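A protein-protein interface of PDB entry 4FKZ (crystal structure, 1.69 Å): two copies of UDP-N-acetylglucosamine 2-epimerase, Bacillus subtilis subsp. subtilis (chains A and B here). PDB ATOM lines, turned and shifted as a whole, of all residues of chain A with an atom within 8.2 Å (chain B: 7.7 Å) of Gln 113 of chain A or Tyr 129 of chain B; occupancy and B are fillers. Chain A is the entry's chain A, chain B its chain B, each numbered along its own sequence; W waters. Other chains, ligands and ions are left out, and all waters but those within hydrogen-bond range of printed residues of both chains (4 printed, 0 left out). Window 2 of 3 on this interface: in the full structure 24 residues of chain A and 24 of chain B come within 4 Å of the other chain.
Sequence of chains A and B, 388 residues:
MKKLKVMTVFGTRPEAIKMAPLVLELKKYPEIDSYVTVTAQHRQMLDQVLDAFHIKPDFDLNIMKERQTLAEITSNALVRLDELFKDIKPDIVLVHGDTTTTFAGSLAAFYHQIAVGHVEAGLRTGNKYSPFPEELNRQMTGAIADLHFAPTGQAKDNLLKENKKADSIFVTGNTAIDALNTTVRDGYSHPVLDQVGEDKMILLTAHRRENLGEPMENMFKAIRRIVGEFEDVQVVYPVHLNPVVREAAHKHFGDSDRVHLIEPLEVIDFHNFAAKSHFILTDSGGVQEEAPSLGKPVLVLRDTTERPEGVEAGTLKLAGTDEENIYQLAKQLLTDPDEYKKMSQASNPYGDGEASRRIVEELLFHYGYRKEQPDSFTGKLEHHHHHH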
ATOM      1  N   PHE A  85     -13.333 -29.058 -26.539  1.00  0.00           N
ATOM      2  CA  PHE A  85     -12.493 -28.559 -27.626  1.00  0.00           C
ATOM      3  C   PHE A  85     -11.749 -29.663 -28.400  1.00  0.00           C
ATOM      4  O   PHE A  85     -11.221 -29.415 -29.494  1.00  0.00           O
ATOM      5  CB  PHE A  85     -11.529 -27.475 -27.120  1.00  0.00           C
ATOM      6  CG  PHE A  85     -12.217 -26.203 -26.687  1.00  0.00           C
ATOM      7  CD1 PHE A  85     -13.330 -25.725 -27.366  1.00  0.00           C
ATOM      8  CD2 PHE A  85     -11.719 -25.459 -25.621  1.00  0.00           C
ATOM      9  CE1 PHE A  85     -13.949 -24.549 -26.970  1.00  0.00           C
ATOM     10  CE2 PHE A  85     -12.329 -24.275 -25.226  1.00  0.00           C
ATOM     11  CZ  PHE A  85     -13.450 -23.821 -25.897  1.00  0.00           C
ATOM     12  N   LYS A  89     -14.087 -27.169 -32.711  1.00  0.00           N
ATOM     13  CA  LYS A  89     -13.069 -26.134 -32.852  1.00  0.00           C
ATOM     14  C   LYS A  89     -13.661 -24.880 -33.480  1.00  0.00           C
ATOM     15  O   LYS A  89     -13.643 -24.729 -34.706  1.00  0.00           O
ATOM     16  CB  LYS A  89     -11.906 -26.621 -33.729  1.00  0.00           C
ATOM     17  CG  LYS A  89     -11.154 -27.838 -33.208  1.00  0.00           C
ATOM     18  CD  LYS A  89     -11.629 -29.130 -33.862  1.00  0.00           C
ATOM     19  CE  LYS A  89     -10.856 -30.328 -33.323  1.00  0.00           C
ATOM     20  NZ  LYS A  89     -11.294 -31.599 -33.967  1.00  0.00           N
ATOM     21  N   PRO A  90     -14.173 -23.957 -32.648  1.00  0.00           N
ATOM     22  CA  PRO A  90     -14.587 -22.676 -33.216  1.00  0.00           C
ATOM     23  C   PRO A  90     -13.384 -21.888 -33.722  1.00  0.00           C
ATOM     24  O   PRO A  90     -12.246 -22.204 -33.363  1.00  0.00           O
ATOM     25  CB  PRO A  90     -15.235 -21.943 -32.030  1.00  0.00           C
ATOM     26  CG  PRO A  90     -14.741 -22.634 -30.810  1.00  0.00           C
ATOM     27  CD  PRO A  90     -14.373 -24.033 -31.190  1.00  0.00           C
ATOM     28  N   ASP A  91     -13.639 -20.877 -34.551  1.00  0.00           N
ATOM     29  CA  ASP A  91     -12.593 -19.958 -34.991  1.00  0.00           C
ATOM     30  C   ASP A  91     -12.188 -19.003 -33.864  1.00  0.00           C
ATOM     31  O   ASP A  91     -11.029 -18.601 -33.759  1.00  0.00           O
ATOM     32  CB  ASP A  91     -13.042 -19.177 -36.224  1.00  0.00           C
ATOM     33  CG  ASP A  91     -13.237 -20.075 -37.433  1.00  0.00           C
ATOM     34  OD1 ASP A  91     -12.311 -20.868 -37.737  1.00  0.00           O
ATOM     35  OD2 ASP A  91     -14.328 -20.029 -38.052  1.00  0.00           O
ATOM     36  N   ILE A  92     -13.147 -18.646 -33.024  1.00  0.00           N
ATOM     37  CA  ILE A  92     -12.870 -17.738 -31.901  1.00  0.00           C
ATOM     38  C   ILE A  92     -13.824 -18.048 -30.768  1.00  0.00           C
ATOM     39  O   ILE A  92     -15.006 -18.351 -30.998  1.00  0.00           O
ATOM     40  CB  ILE A  92     -12.906 -16.233 -32.319  1.00  0.00           C
ATOM     41  CG1 ILE A  92     -12.427 -15.310 -31.174  1.00  0.00           C
ATOM     42  CG2 ILE A  92     -14.283 -15.835 -32.857  1.00  0.00           C
ATOM     43  CD1 ILE A  92     -12.054 -13.905 -31.631  1.00  0.00           C
ATOM     44  N   SER A 106     -10.782 -19.135 -21.269  1.00  0.00           N
ATOM     45  CA  SER A 106      -9.670 -18.570 -22.024  1.00  0.00           C
ATOM     46  C   SER A 106      -8.497 -19.537 -22.083  1.00  0.00           C
ATOM     47  O   SER A 106      -7.860 -19.710 -23.122  1.00  0.00           O
ATOM     48  CB  SER A 106      -9.197 -17.284 -21.334  1.00  0.00           C
ATOM     49  OG  SER A 106     -10.227 -16.333 -21.428  1.00  0.00           O
ATOM     50  N   LEU A 107      -8.216 -20.147 -20.944  1.00  0.00           N
ATOM     51  CA  LEU A 107      -7.072 -21.047 -20.818  1.00  0.00           C
ATOM     52  C   LEU A 107      -7.307 -22.315 -21.636  1.00  0.00           C
ATOM     53  O   LEU A 107      -6.406 -22.787 -22.338  1.00  0.00           O
ATOM     54  CB  LEU A 107      -6.824 -21.397 -19.347  1.00  0.00           C
ATOM     55  CG  LEU A 107      -5.525 -22.154 -19.009  1.00  0.00           C
ATOM     56  CD1 LEU A 107      -4.275 -21.318 -19.300  1.00  0.00           C
ATOM     57  CD2 LEU A 107      -5.564 -22.618 -17.552  1.00  0.00           C
ATOM     58  N   ALA A 108      -8.515 -22.862 -21.548  1.00  0.00           N
ATOM     59  CA  ALA A 108      -8.845 -24.068 -22.325  1.00  0.00           C
ATOM     60  C   ALA A 108      -8.741 -23.797 -23.832  1.00  0.00           C
ATOM     61  O   ALA A 108      -8.170 -24.618 -24.582  1.00  0.00           O
ATOM     62  CB  ALA A 108     -10.228 -24.580 -21.957  1.00  0.00           C
ATOM     63  N   ALA A 109      -9.261 -22.644 -24.278  1.00  0.00           N
ATOM     64  CA  ALA A 109      -9.143 -22.240 -25.682  1.00  0.00           C
ATOM     65  C   ALA A 109      -7.680 -22.116 -26.096  1.00  0.00           C
ATOM     66  O   ALA A 109      -7.264 -22.655 -27.127  1.00  0.00           O
ATOM     67  CB  ALA A 109      -9.902 -20.932 -25.940  1.00  0.00           C
ATOM     68  N   PHE A 110      -6.887 -21.437 -25.263  1.00  0.00           N
ATOM     69  CA  PHE A 110      -5.463 -21.287 -25.530  1.00  0.00           C
ATOM     70  C   PHE A 110      -4.738 -22.641 -25.677  1.00  0.00           C
ATOM     71  O   PHE A 110      -3.907 -22.795 -26.578  1.00  0.00           O
ATOM     72  CB  PHE A 110      -4.821 -20.436 -24.433  1.00  0.00           C
ATOM     73  CG  PHE A 110      -3.325 -20.394 -24.500  1.00  0.00           C
ATOM     74  CD1 PHE A 110      -2.670 -19.856 -25.614  1.00  0.00           C
ATOM     75  CD2 PHE A 110      -2.573 -20.923 -23.465  1.00  0.00           C
ATOM     76  CE1 PHE A 110      -1.274 -19.834 -25.665  1.00  0.00           C
ATOM     77  CE2 PHE A 110      -1.180 -20.904 -23.512  1.00  0.00           C
ATOM     78  CZ  PHE A 110      -0.538 -20.365 -24.612  1.00  0.00           C
ATOM     79  N   TYR A 111      -5.079 -23.598 -24.813  1.00  0.00           N
ATOM     80  CA  TYR A 111      -4.442 -24.928 -24.847  1.00  0.00           C
ATOM     81  C   TYR A 111      -4.723 -25.649 -26.168  1.00  0.00           C
ATOM     82  O   TYR A 111      -3.967 -26.550 -26.567  1.00  0.00           O
ATOM     83  CB  TYR A 111      -4.868 -25.795 -23.645  1.00  0.00           C
ATOM     84  CG  TYR A 111      -4.233 -25.411 -22.302  1.00  0.00           C
ATOM     85  CD1 TYR A 111      -3.184 -24.480 -22.234  1.00  0.00           C
ATOM     86  CD2 TYR A 111      -4.656 -26.014 -21.112  1.00  0.00           C
ATOM     87  CE1 TYR A 111      -2.595 -24.149 -21.014  1.00  0.00           C
ATOM     88  CE2 TYR A 111      -4.065 -25.705 -19.893  1.00  0.00           C
ATOM     89  CZ  TYR A 111      -3.040 -24.770 -19.853  1.00  0.00           C
ATOM     90  OH  TYR A 111      -2.469 -24.447 -18.641  1.00  0.00           O
ATOM     91  N   HIS A 112      -5.805 -25.253 -26.844  1.00  0.00           N
ATOM     92  CA  HIS A 112      -6.155 -25.784 -28.157  1.00  0.00           C
ATOM     93  C   HIS A 112      -5.859 -24.846 -29.301  1.00  0.00           C
ATOM     94  O   HIS A 112      -6.287 -25.080 -30.452  1.00  0.00           O
ATOM     95  CB  HIS A 112      -7.621 -26.203 -28.144  1.00  0.00           C
ATOM     96  CG  HIS A 112      -7.856 -27.494 -27.411  1.00  0.00           C
ATOM     97  ND1 HIS A 112      -8.059 -27.554 -26.075  1.00  0.00           N
ATOM     98  CD2 HIS A 112      -7.861 -28.812 -27.871  1.00  0.00           C
ATOM     99  CE1 HIS A 112      -8.209 -28.841 -25.708  1.00  0.00           C
ATOM    100  NE2 HIS A 112      -8.085 -29.609 -26.808  1.00  0.00           N
ATOM    101  N   GLN A 113      -5.111 -23.785 -28.997  1.00  0.00           N
ATOM    102  CA  GLN A 113      -4.721 -22.772 -29.968  1.00  0.00           C
ATOM    103  C   GLN A 113      -5.939 -22.186 -30.695  1.00  0.00           C
ATOM    104  O   GLN A 113      -5.903 -21.949 -31.904  1.00  0.00           O
ATOM    105  CB  GLN A 113      -3.649 -23.307 -30.937  1.00  0.00           C
ATOM    106  CG  GLN A 113      -2.434 -23.848 -30.186  1.00  0.00           C
ATOM    107  CD  GLN A 113      -1.165 -23.887 -31.021  1.00  0.00           C
ATOM    108  OE1 GLN A 113      -1.216 -23.958 -32.251  1.00  0.00           O
ATOM    109  NE2 GLN A 113      -0.004 -23.853 -30.345  1.00  0.00           N
ATOM    110  N   ILE A 114      -6.999 -21.956 -29.926  1.00  0.00           N
ATOM    111  CA  ILE A 114      -8.216 -21.292 -30.418  1.00  0.00           C
ATOM    112  C   ILE A 114      -8.137 -19.823 -30.004  1.00  0.00           C
ATOM    113  O   ILE A 114      -7.843 -19.508 -28.830  1.00  0.00           O
ATOM    114  CB  ILE A 114      -9.501 -21.938 -29.831  1.00  0.00           C
ATOM    115  CG1 ILE A 114      -9.648 -23.395 -30.301  1.00  0.00           C
ATOM    116  CG2 ILE A 114     -10.757 -21.147 -30.214  1.00  0.00           C
ATOM    117  CD1 ILE A 114     -10.636 -24.212 -29.480  1.00  0.00           C
ATOM    118  N   ALA A 115      -8.395 -18.935 -30.967  1.00  0.00           N
ATOM    119  CA  ALA A 115      -8.403 -17.488 -30.700  1.00  0.00           C
ATOM    120  C   ALA A 115      -9.429 -17.103 -29.627  1.00  0.00           C
ATOM    121  O   ALA A 115     -10.466 -17.753 -29.481  1.00  0.00           O
ATOM    122  CB  ALA A 115      -8.643 -16.711 -31.991  1.00  0.00           C
ATOM    123  N   VAL A 116      -9.119 -16.053 -28.866  1.00  0.00           N
ATOM    124  CA  VAL A 116      -9.980 -15.617 -27.764  1.00  0.00           C
ATOM    125  C   VAL A 116     -10.275 -14.129 -27.903  1.00  0.00           C
ATOM    126  O   VAL A 116      -9.349 -13.325 -28.101  1.00  0.00           O
ATOM    127  CB  VAL A 116      -9.332 -15.888 -26.376  1.00  0.00           C
ATOM    128  CG1 VAL A 116     -10.141 -15.253 -25.247  1.00  0.00           C
ATOM    129  CG2 VAL A 116      -9.186 -17.386 -26.136  1.00  0.00           C
ATOM    130  N   ILE A 144      -4.077 -13.833 -22.336  1.00  0.00           N
ATOM    131  CA  ILE A 144      -4.465 -14.812 -23.367  1.00  0.00           C
ATOM    132  C   ILE A 144      -5.191 -14.164 -24.558  1.00  0.00           C
ATOM    133  O   ILE A 144      -4.958 -14.529 -25.712  1.00  0.00           O
ATOM    134  CB  ILE A 144      -5.372 -15.907 -22.765  1.00  0.00           C
ATOM    135  CG1 ILE A 144      -4.604 -16.747 -21.751  1.00  0.00           C
ATOM    136  CG2 ILE A 144      -5.956 -16.822 -23.854  1.00  0.00           C
ATOM    137  CD1 ILE A 144      -5.485 -17.599 -20.868  1.00  0.00           C
ATOM    138  N   ASP A 146      -6.752 -12.356 -27.722  1.00  0.00           N
ATOM    139  CA  ASP A 146      -6.255 -11.800 -28.979  1.00  0.00           C
ATOM    140  C   ASP A 146      -6.947 -10.491 -29.290  1.00  0.00           C
ATOM    141  O   ASP A 146      -6.345  -9.582 -29.859  1.00  0.00           O
ATOM    142  CB  ASP A 146      -6.534 -12.776 -30.125  1.00  0.00           C
ATOM    143  CG  ASP A 146      -5.812 -14.087 -29.939  1.00  0.00           C
ATOM    144  OD1 ASP A 146      -4.564 -14.080 -29.956  1.00  0.00           O
ATOM    145  OD2 ASP A 146      -6.478 -15.109 -29.705  1.00  0.00           O
ATOM    146  N   LEU B  70      -1.697 -30.440 -21.546  1.00  0.00           N
ATOM    147  CA  LEU B  70      -1.629 -29.198 -20.762  1.00  0.00           C
ATOM    148  C   LEU B  70      -2.747 -29.091 -19.723  1.00  0.00           C
ATOM    149  O   LEU B  70      -2.495 -28.741 -18.558  1.00  0.00           O
ATOM    150  CB  LEU B  70      -1.604 -27.975 -21.695  1.00  0.00           C
ATOM    151  CG  LEU B  70      -0.386 -27.887 -22.628  1.00  0.00           C
ATOM    152  CD1 LEU B  70      -0.500 -26.670 -23.541  1.00  0.00           C
ATOM    153  CD2 LEU B  70       0.946 -27.876 -21.868  1.00  0.00           C
ATOM    154  N   THR B 125       9.125 -13.452 -25.668  1.00  0.00           N
ATOM    155  CA  THR B 125       9.280 -13.407 -27.125  1.00  0.00           C
ATOM    156  C   THR B 125       8.207 -12.532 -27.749  1.00  0.00           C
ATOM    157  O   THR B 125       8.330 -12.128 -28.905  1.00  0.00           O
ATOM    158  CB  THR B 125       9.118 -14.790 -27.780  1.00  0.00           C
ATOM    159  OG1 THR B 125       7.825 -15.322 -27.465  1.00  0.00           O
ATOM    160  CG2 THR B 125      10.201 -15.745 -27.313  1.00  0.00           C
ATOM    161  N   GLY B 126       7.137 -12.284 -27.001  1.00  0.00           N
ATOM    162  CA  GLY B 126       5.977 -11.561 -27.534  1.00  0.00           C
ATOM    163  C   GLY B 126       5.048 -12.415 -28.388  1.00  0.00           C
ATOM    164  O   GLY B 126       4.041 -11.917 -28.911  1.00  0.00           O
ATOM    165  N   ASN B 127       5.368 -13.704 -28.521  1.00  0.00           N
ATOM    166  CA  ASN B 127       4.617 -14.615 -29.382  1.00  0.00           C
ATOM    167  C   ASN B 127       3.956 -15.726 -28.552  1.00  0.00           C
ATOM    168  O   ASN B 127       4.643 -16.609 -28.002  1.00  0.00           O
ATOM    169  CB  ASN B 127       5.561 -15.190 -30.448  1.00  0.00           C
ATOM    170  CG  ASN B 127       4.849 -16.044 -31.488  1.00  0.00           C
ATOM    171  OD1 ASN B 127       3.858 -16.719 -31.205  1.00  0.00           O
ATOM    172  ND2 ASN B 127       5.372 -16.023 -32.713  1.00  0.00           N
ATOM    173  N   LYS B 128       2.625 -15.678 -28.444  1.00  0.00           N
ATOM    174  CA  LYS B 128       1.887 -16.603 -27.568  1.00  0.00           C
ATOM    175  C   LYS B 128       1.961 -18.070 -28.001  1.00  0.00           C
ATOM    176  O   LYS B 128       1.577 -18.978 -27.257  1.00  0.00           O
ATOM    177  CB  LYS B 128       0.411 -16.155 -27.409  1.00  0.00           C
ATOM    178  CG  LYS B 128      -0.429 -16.351 -28.672  1.00  0.00           C
ATOM    179  CD  LYS B 128      -1.820 -15.716 -28.583  1.00  0.00           C
ATOM    180  CE  LYS B 128      -2.796 -16.615 -27.833  1.00  0.00           C
ATOM    181  NZ  LYS B 128      -4.215 -16.133 -27.874  1.00  0.00           N
ATOM    182  N   TYR B 129       2.429 -18.309 -29.220  1.00  0.00           N
ATOM    183  CA  TYR B 129       2.553 -19.681 -29.694  1.00  0.00           C
ATOM    184  C   TYR B 129       4.014 -20.108 -29.925  1.00  0.00           C
ATOM    185  O   TYR B 129       4.289 -21.170 -30.503  1.00  0.00           O
ATOM    186  CB  TYR B 129       1.688 -19.892 -30.940  1.00  0.00           C
ATOM    187  CG  TYR B 129       0.192 -19.708 -30.716  1.00  0.00           C
ATOM    188  CD1 TYR B 129      -0.472 -20.359 -29.670  1.00  0.00           C
ATOM    189  CD2 TYR B 129      -0.563 -18.917 -31.580  1.00  0.00           C
ATOM    190  CE1 TYR B 129      -1.847 -20.208 -29.490  1.00  0.00           C
ATOM    191  CE2 TYR B 129      -1.936 -18.758 -31.405  1.00  0.00           C
ATOM    192  CZ  TYR B 129      -2.574 -19.404 -30.361  1.00  0.00           C
ATOM    193  OH  TYR B 129      -3.936 -19.247 -30.199  1.00  0.00           O
ATOM    194  N   SER B 130       4.951 -19.280 -29.466  1.00  0.00           N
ATOM    195  CA  SER B 130       6.378 -19.604 -29.610  1.00  0.00           C
ATOM    196  C   SER B 130       7.219 -18.868 -28.564  1.00  0.00           C
ATOM    197  O   SER B 130       7.536 -17.695 -28.762  1.00  0.00           O
ATOM    198  CB  SER B 130       6.870 -19.280 -31.034  1.00  0.00           C
ATOM    199  OG  SER B 130       8.269 -19.556 -31.162  1.00  0.00           O
ATOM    200  N   PRO B 131       7.578 -19.551 -27.454  1.00  0.00           N
ATOM    201  CA  PRO B 131       7.275 -20.957 -27.167  1.00  0.00           C
ATOM    202  C   PRO B 131       5.866 -21.170 -26.600  1.00  0.00           C
ATOM    203  O   PRO B 131       5.345 -20.307 -25.897  1.00  0.00           O
ATOM    204  CB  PRO B 131       8.322 -21.333 -26.107  1.00  0.00           C
ATOM    205  CG  PRO B 131       8.613 -20.038 -25.386  1.00  0.00           C
ATOM    206  CD  PRO B 131       8.286 -18.902 -26.327  1.00  0.00           C
ATOM    207  N   PHE B 132       5.288 -22.331 -26.903  1.00  0.00           N
ATOM    208  CA  PHE B 132       3.941 -22.693 -26.476  1.00  0.00           C
ATOM    209  C   PHE B 132       3.986 -23.865 -25.498  1.00  0.00           C
ATOM    210  O   PHE B 132       4.504 -24.938 -25.853  1.00  0.00           O
ATOM    211  CB  PHE B 132       3.112 -23.085 -27.714  1.00  0.00           C
ATOM    212  CG  PHE B 132       1.744 -23.631 -27.387  1.00  0.00           C
ATOM    213  CD1 PHE B 132       0.718 -22.776 -27.003  1.00  0.00           C
ATOM    214  CD2 PHE B 132       1.480 -24.994 -27.470  1.00  0.00           C
ATOM    215  CE1 PHE B 132      -0.544 -23.271 -26.692  1.00  0.00           C
ATOM    216  CE2 PHE B 132       0.225 -25.504 -27.154  1.00  0.00           C
ATOM    217  CZ  PHE B 132      -0.797 -24.635 -26.774  1.00  0.00           C
ATOM    218  N   PRO B 133       3.424 -23.700 -24.278  1.00  0.00           N
ATOM    219  CA  PRO B 133       2.700 -22.558 -23.684  1.00  0.00           C
ATOM    220  C   PRO B 133       3.591 -21.674 -22.798  1.00  0.00           C
ATOM    221  O   PRO B 133       3.072 -20.891 -21.978  1.00  0.00           O
ATOM    222  CB  PRO B 133       1.689 -23.257 -22.785  1.00  0.00           C
ATOM    223  CG  PRO B 133       2.465 -24.437 -22.247  1.00  0.00           C
ATOM    224  CD  PRO B 133       3.361 -24.879 -23.392  1.00  0.00           C
ATOM    225  N   GLU B 134       4.907 -21.817 -22.925  1.00  0.00           N
ATOM    226  CA  GLU B 134       5.811 -21.166 -21.963  1.00  0.00           C
ATOM    227  C   GLU B 134       5.670 -19.646 -21.914  1.00  0.00           C
ATOM    228  O   GLU B 134       5.709 -19.060 -20.818  1.00  0.00           O
ATOM    229  CB  GLU B 134       7.266 -21.567 -22.206  1.00  0.00           C
ATOM    230  CG  GLU B 134       7.561 -23.018 -21.842  1.00  0.00           C
ATOM    231  CD  GLU B 134       7.224 -24.024 -22.936  1.00  0.00           C
ATOM    232  OE1 GLU B 134       6.687 -23.647 -24.012  1.00  0.00           O
ATOM    233  OE2 GLU B 134       7.515 -25.221 -22.707  1.00  0.00           O
ATOM    234  N   GLU B 135       5.517 -19.018 -23.081  1.00  0.00           N
ATOM    235  CA  GLU B 135       5.337 -17.556 -23.122  1.00  0.00           C
ATOM    236  C   GLU B 135       4.143 -17.110 -22.251  1.00  0.00           C
ATOM    237  O   GLU B 135       4.264 -16.178 -21.447  1.00  0.00           O
ATOM    238  CB  GLU B 135       5.237 -17.032 -24.573  1.00  0.00           C
ATOM    239  CG  GLU B 135       4.949 -15.531 -24.689  1.00  0.00           C
ATOM    240  CD  GLU B 135       6.158 -14.637 -24.441  1.00  0.00           C
ATOM    241  OE1 GLU B 135       7.248 -15.129 -24.090  1.00  0.00           O
ATOM    242  OE2 GLU B 135       6.011 -13.409 -24.600  1.00  0.00           O
ATOM    243  N   LEU B 136       2.994 -17.765 -22.380  1.00  0.00           N
ATOM    244  CA  LEU B 136       1.885 -17.380 -21.517  1.00  0.00           C
ATOM    245  C   LEU B 136       2.046 -17.841 -20.070  1.00  0.00           C
ATOM    246  O   LEU B 136       1.604 -17.153 -19.164  1.00  0.00           O
ATOM    247  CB  LEU B 136       0.516 -17.762 -22.121  1.00  0.00           C
ATOM    248  CG  LEU B 136       0.096 -17.005 -23.404  1.00  0.00           C
ATOM    249  CD1 LEU B 136      -1.414 -16.962 -23.437  1.00  0.00           C
ATOM    250  CD2 LEU B 136       0.636 -15.583 -23.537  1.00  0.00           C
ATOM    251  N   ARG B 209       7.606 -27.906 -27.528  1.00  0.00           N
ATOM    252  CA  ARG B 209       6.255 -28.361 -27.899  1.00  0.00           C
ATOM    253  C   ARG B 209       5.837 -27.912 -29.311  1.00  0.00           C
ATOM    254  O   ARG B 209       5.317 -28.726 -30.090  1.00  0.00           O
ATOM    255  CB  ARG B 209       5.250 -27.899 -26.839  1.00  0.00           C
ATOM    256  CG  ARG B 209       3.843 -28.486 -26.922  1.00  0.00           C
ATOM    257  CD  ARG B 209       3.054 -28.074 -25.674  1.00  0.00           C
ATOM    258  NE  ARG B 209       3.790 -28.458 -24.472  1.00  0.00           N
ATOM    259  CZ  ARG B 209       3.546 -29.535 -23.728  1.00  0.00           C
ATOM    260  NH1 ARG B 209       2.526 -30.349 -24.011  1.00  0.00           N
ATOM    261  NH2 ARG B 209       4.326 -29.795 -22.678  1.00  0.00           N
ATOM    262  N   GLU B 210       6.093 -26.650 -29.655  1.00  0.00           N
ATOM    263  CA  GLU B 210       5.743 -26.108 -30.974  1.00  0.00           C
ATOM    264  C   GLU B 210       6.639 -26.662 -32.097  1.00  0.00           C
ATOM    265  O   GLU B 210       6.341 -26.474 -33.277  1.00  0.00           O
ATOM    266  CB  GLU B 210       5.757 -24.570 -30.964  1.00  0.00           C
ATOM    267  CG  GLU B 210       7.129 -23.947 -30.761  1.00  0.00           C
ATOM    268  CD  GLU B 210       7.571 -23.867 -29.307  1.00  0.00           C
ATOM    269  OE1 GLU B 210       6.864 -24.372 -28.397  1.00  0.00           O
ATOM    270  OE2 GLU B 210       8.665 -23.294 -29.080  1.00  0.00           O
ATOM    271  N   ASN B 211       7.730 -27.335 -31.729  1.00  0.00           N
ATOM    272  CA  ASN B 211       8.608 -27.972 -32.723  1.00  0.00           C
ATOM    273  C   ASN B 211       8.289 -29.432 -33.003  1.00  0.00           C
ATOM    274  O   ASN B 211       8.848 -30.009 -33.934  1.00  0.00           O
ATOM    275  CB  ASN B 211      10.082 -27.865 -32.309  1.00  0.00           C
ATOM    276  CG  ASN B 211      10.643 -26.470 -32.493  1.00  0.00           C
ATOM    277  OD1 ASN B 211      10.069 -25.649 -33.196  1.00  0.00           O
ATOM    278  ND2 ASN B 211      11.777 -26.194 -31.849  1.00  0.00           N
ATOM    279  N   ASP B 303      12.083 -20.415 -34.202  1.00  0.00           N
ATOM    280  CA  ASP B 303      11.825 -19.167 -34.912  1.00  0.00           C
ATOM    281  C   ASP B 303      11.893 -17.919 -34.012  1.00  0.00           C
ATOM    282  O   ASP B 303      11.850 -16.791 -34.506  1.00  0.00           O
ATOM    283  CB  ASP B 303      10.509 -19.234 -35.716  1.00  0.00           C
ATOM    284  CG  ASP B 303       9.261 -19.393 -34.842  1.00  0.00           C
ATOM    285  OD1 ASP B 303       9.361 -19.632 -33.615  1.00  0.00           O
ATOM    286  OD2 ASP B 303       8.149 -19.285 -35.414  1.00  0.00           O
ATOM    287  N   THR B 304      11.983 -18.138 -32.699  1.00  0.00           N
ATOM    288  CA  THR B 304      12.092 -17.061 -31.704  1.00  0.00           C
ATOM    289  C   THR B 304      13.086 -17.440 -30.604  1.00  0.00           C
ATOM    290  O   THR B 304      13.349 -18.617 -30.380  1.00  0.00           O
ATOM    291  CB  THR B 304      10.748 -16.788 -30.968  1.00  0.00           C
ATOM    292  OG1 THR B 304      10.361 -17.944 -30.203  1.00  0.00           O
ATOM    293  CG2 THR B 304       9.632 -16.412 -31.945  1.00  0.00           C
HETATM  294  O   HOH W   1       2.693 -23.284 -31.566  1.00  0.00           O
HETATM  295  O   HOH W   2      -4.926 -17.058 -31.412  1.00  0.00           O
HETATM  296  O   HOH W   3      -5.429 -18.757 -27.931  1.00  0.00           O
HETATM  297  O   HOH W   4      -5.067 -19.346 -33.187  1.00  0.00           O
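O of Ile 144 of chain A sits at hydrogen-bond distance from NZ of Lys 128 of chain B, at 2.8 Å. The side-chain amino group of Lys 128 of chain B is in salt-bridge range of the side-chain carboxylate of Asp 146 of chain A (2.9 Å).
The backbone NH of Phe 132 of chain B sits at hydrogen-bond distance from the side-chain carboxylate of Glu 210 of chain B (3.0 Å). The backbone NH (N) of Tyr 129 of chain B lies within hydrogen-bond range of the side-chain amide oxygen (OD1) of Asn 127 of chain B (2.9 Å). The backbone NH (N) of Asp 146 of chain A sits at hydrogen-bond distance from the backbone carbonyl oxygen (O) of Val 116 of chain A (2.8 Å). OE1 of Glu 134 of chain B sits close to N of Phe 132 of chain B (3.5 Å).
CE1 of Phe 110 of chain A touches O of Lys 128 of chain B, at 3.4 Å. CE1 of Tyr 129 of chain B touches CE1 of Phe 110 of chain A, 3.9 Å away. O of Phe 110 of chain A touches CE1 of Phe 132 of chain B, 3.4 Å away. CB of Pro 133 of chain B touches CE2 of Phe 110 of chain A (3.8 Å). Phe 110 of chain A touches Leu 136 of chain B. C of Leu 70 of chain B touches CE2 of Tyr 111 of chain A (3.6 Å). Phe 132 of chain B touches Tyr 111 of chain A. Gln 113 of chain A touches Tyr 129 of chain B (NE2 to CD1, 3.6 Å). Phe 132 of chain B touches Gln 113 of chain A. CG1 of Ile 144 of chain A touches CD1 of Leu 136 of chain B, 3.6 Å away.
Of chain B, only Tyr 129 (3.6 Å) and Phe 132 (3.4 Å) come within 4 Å of Gln 113 of chain A. Tyr 129 of chain B touches just these residues of chain A: Phe 110 and Gln 113. Printed residues of chain B within 4 Å of Tyr 111 of chain A: Leu 70 and Phe 132. Of the printed residues of chain A, Lys 128 of chain B touches Phe 110 (3.4 Å), Ile 144 (2.8 Å) and Asp 146 (2.9 Å). Of the printed residues of chain B, Asp 146 of chain A touches Lys 128 (2.9 Å). Of the printed residues of chain A, Leu 70 of chain B touches Tyr 111 (3.6 Å). Of the printed residues of chain A, Phe 132 of chain B touches Phe 110 (3.4 Å), Tyr 111 (3.7 Å) and Gln 113 (3.4 Å). The nearest residue of chain B that does not touch Gln 113 of chain A is Glu 210 of chain B (5.8 Å). The nearest printed residue of chain A that does not touch Pro 133 of chain B is Tyr 111 of chain A (4.7 Å).
Hydrophobic or aromatic side chains of chain B within 4 Å of the printed part of chain A: Leu 70, Tyr 129, Phe 132, Pro 133 and Leu 136. Among the printed residues, 12 pairs touch across the chains. Among the printed residues, Asp or Glu carboxylates within 4 Å of a Lys or Arg side-chain nitrogen of the other chain: Asp 146 of chain A with Lys 128 of chain B.
No position is printed for both chains.
Water W3 lies within hydrogen-bond range of O of Ile 114 of chain A (2.7 Å), OH of Tyr 129 of chain B (2.8 Å) and NZ of Lys 128 of chain B (2.9 Å). Water W2 bridges OH of Tyr 129 of chain B (2.7 Å) and OD2 of Asp 146 of chain A (3.0 Å). Water W1 bridges O of Tyr 129 of chain B (2.9 Å) and NE2 of Gln 113 of chain A (3.0 Å). Water W4 lies within hydrogen-bond range of the backbone carbonyl oxygen of Gln 113 of chain A (3.0 Å) and the side-chain hydroxyl of Tyr 129 of chain B (3.2 Å).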
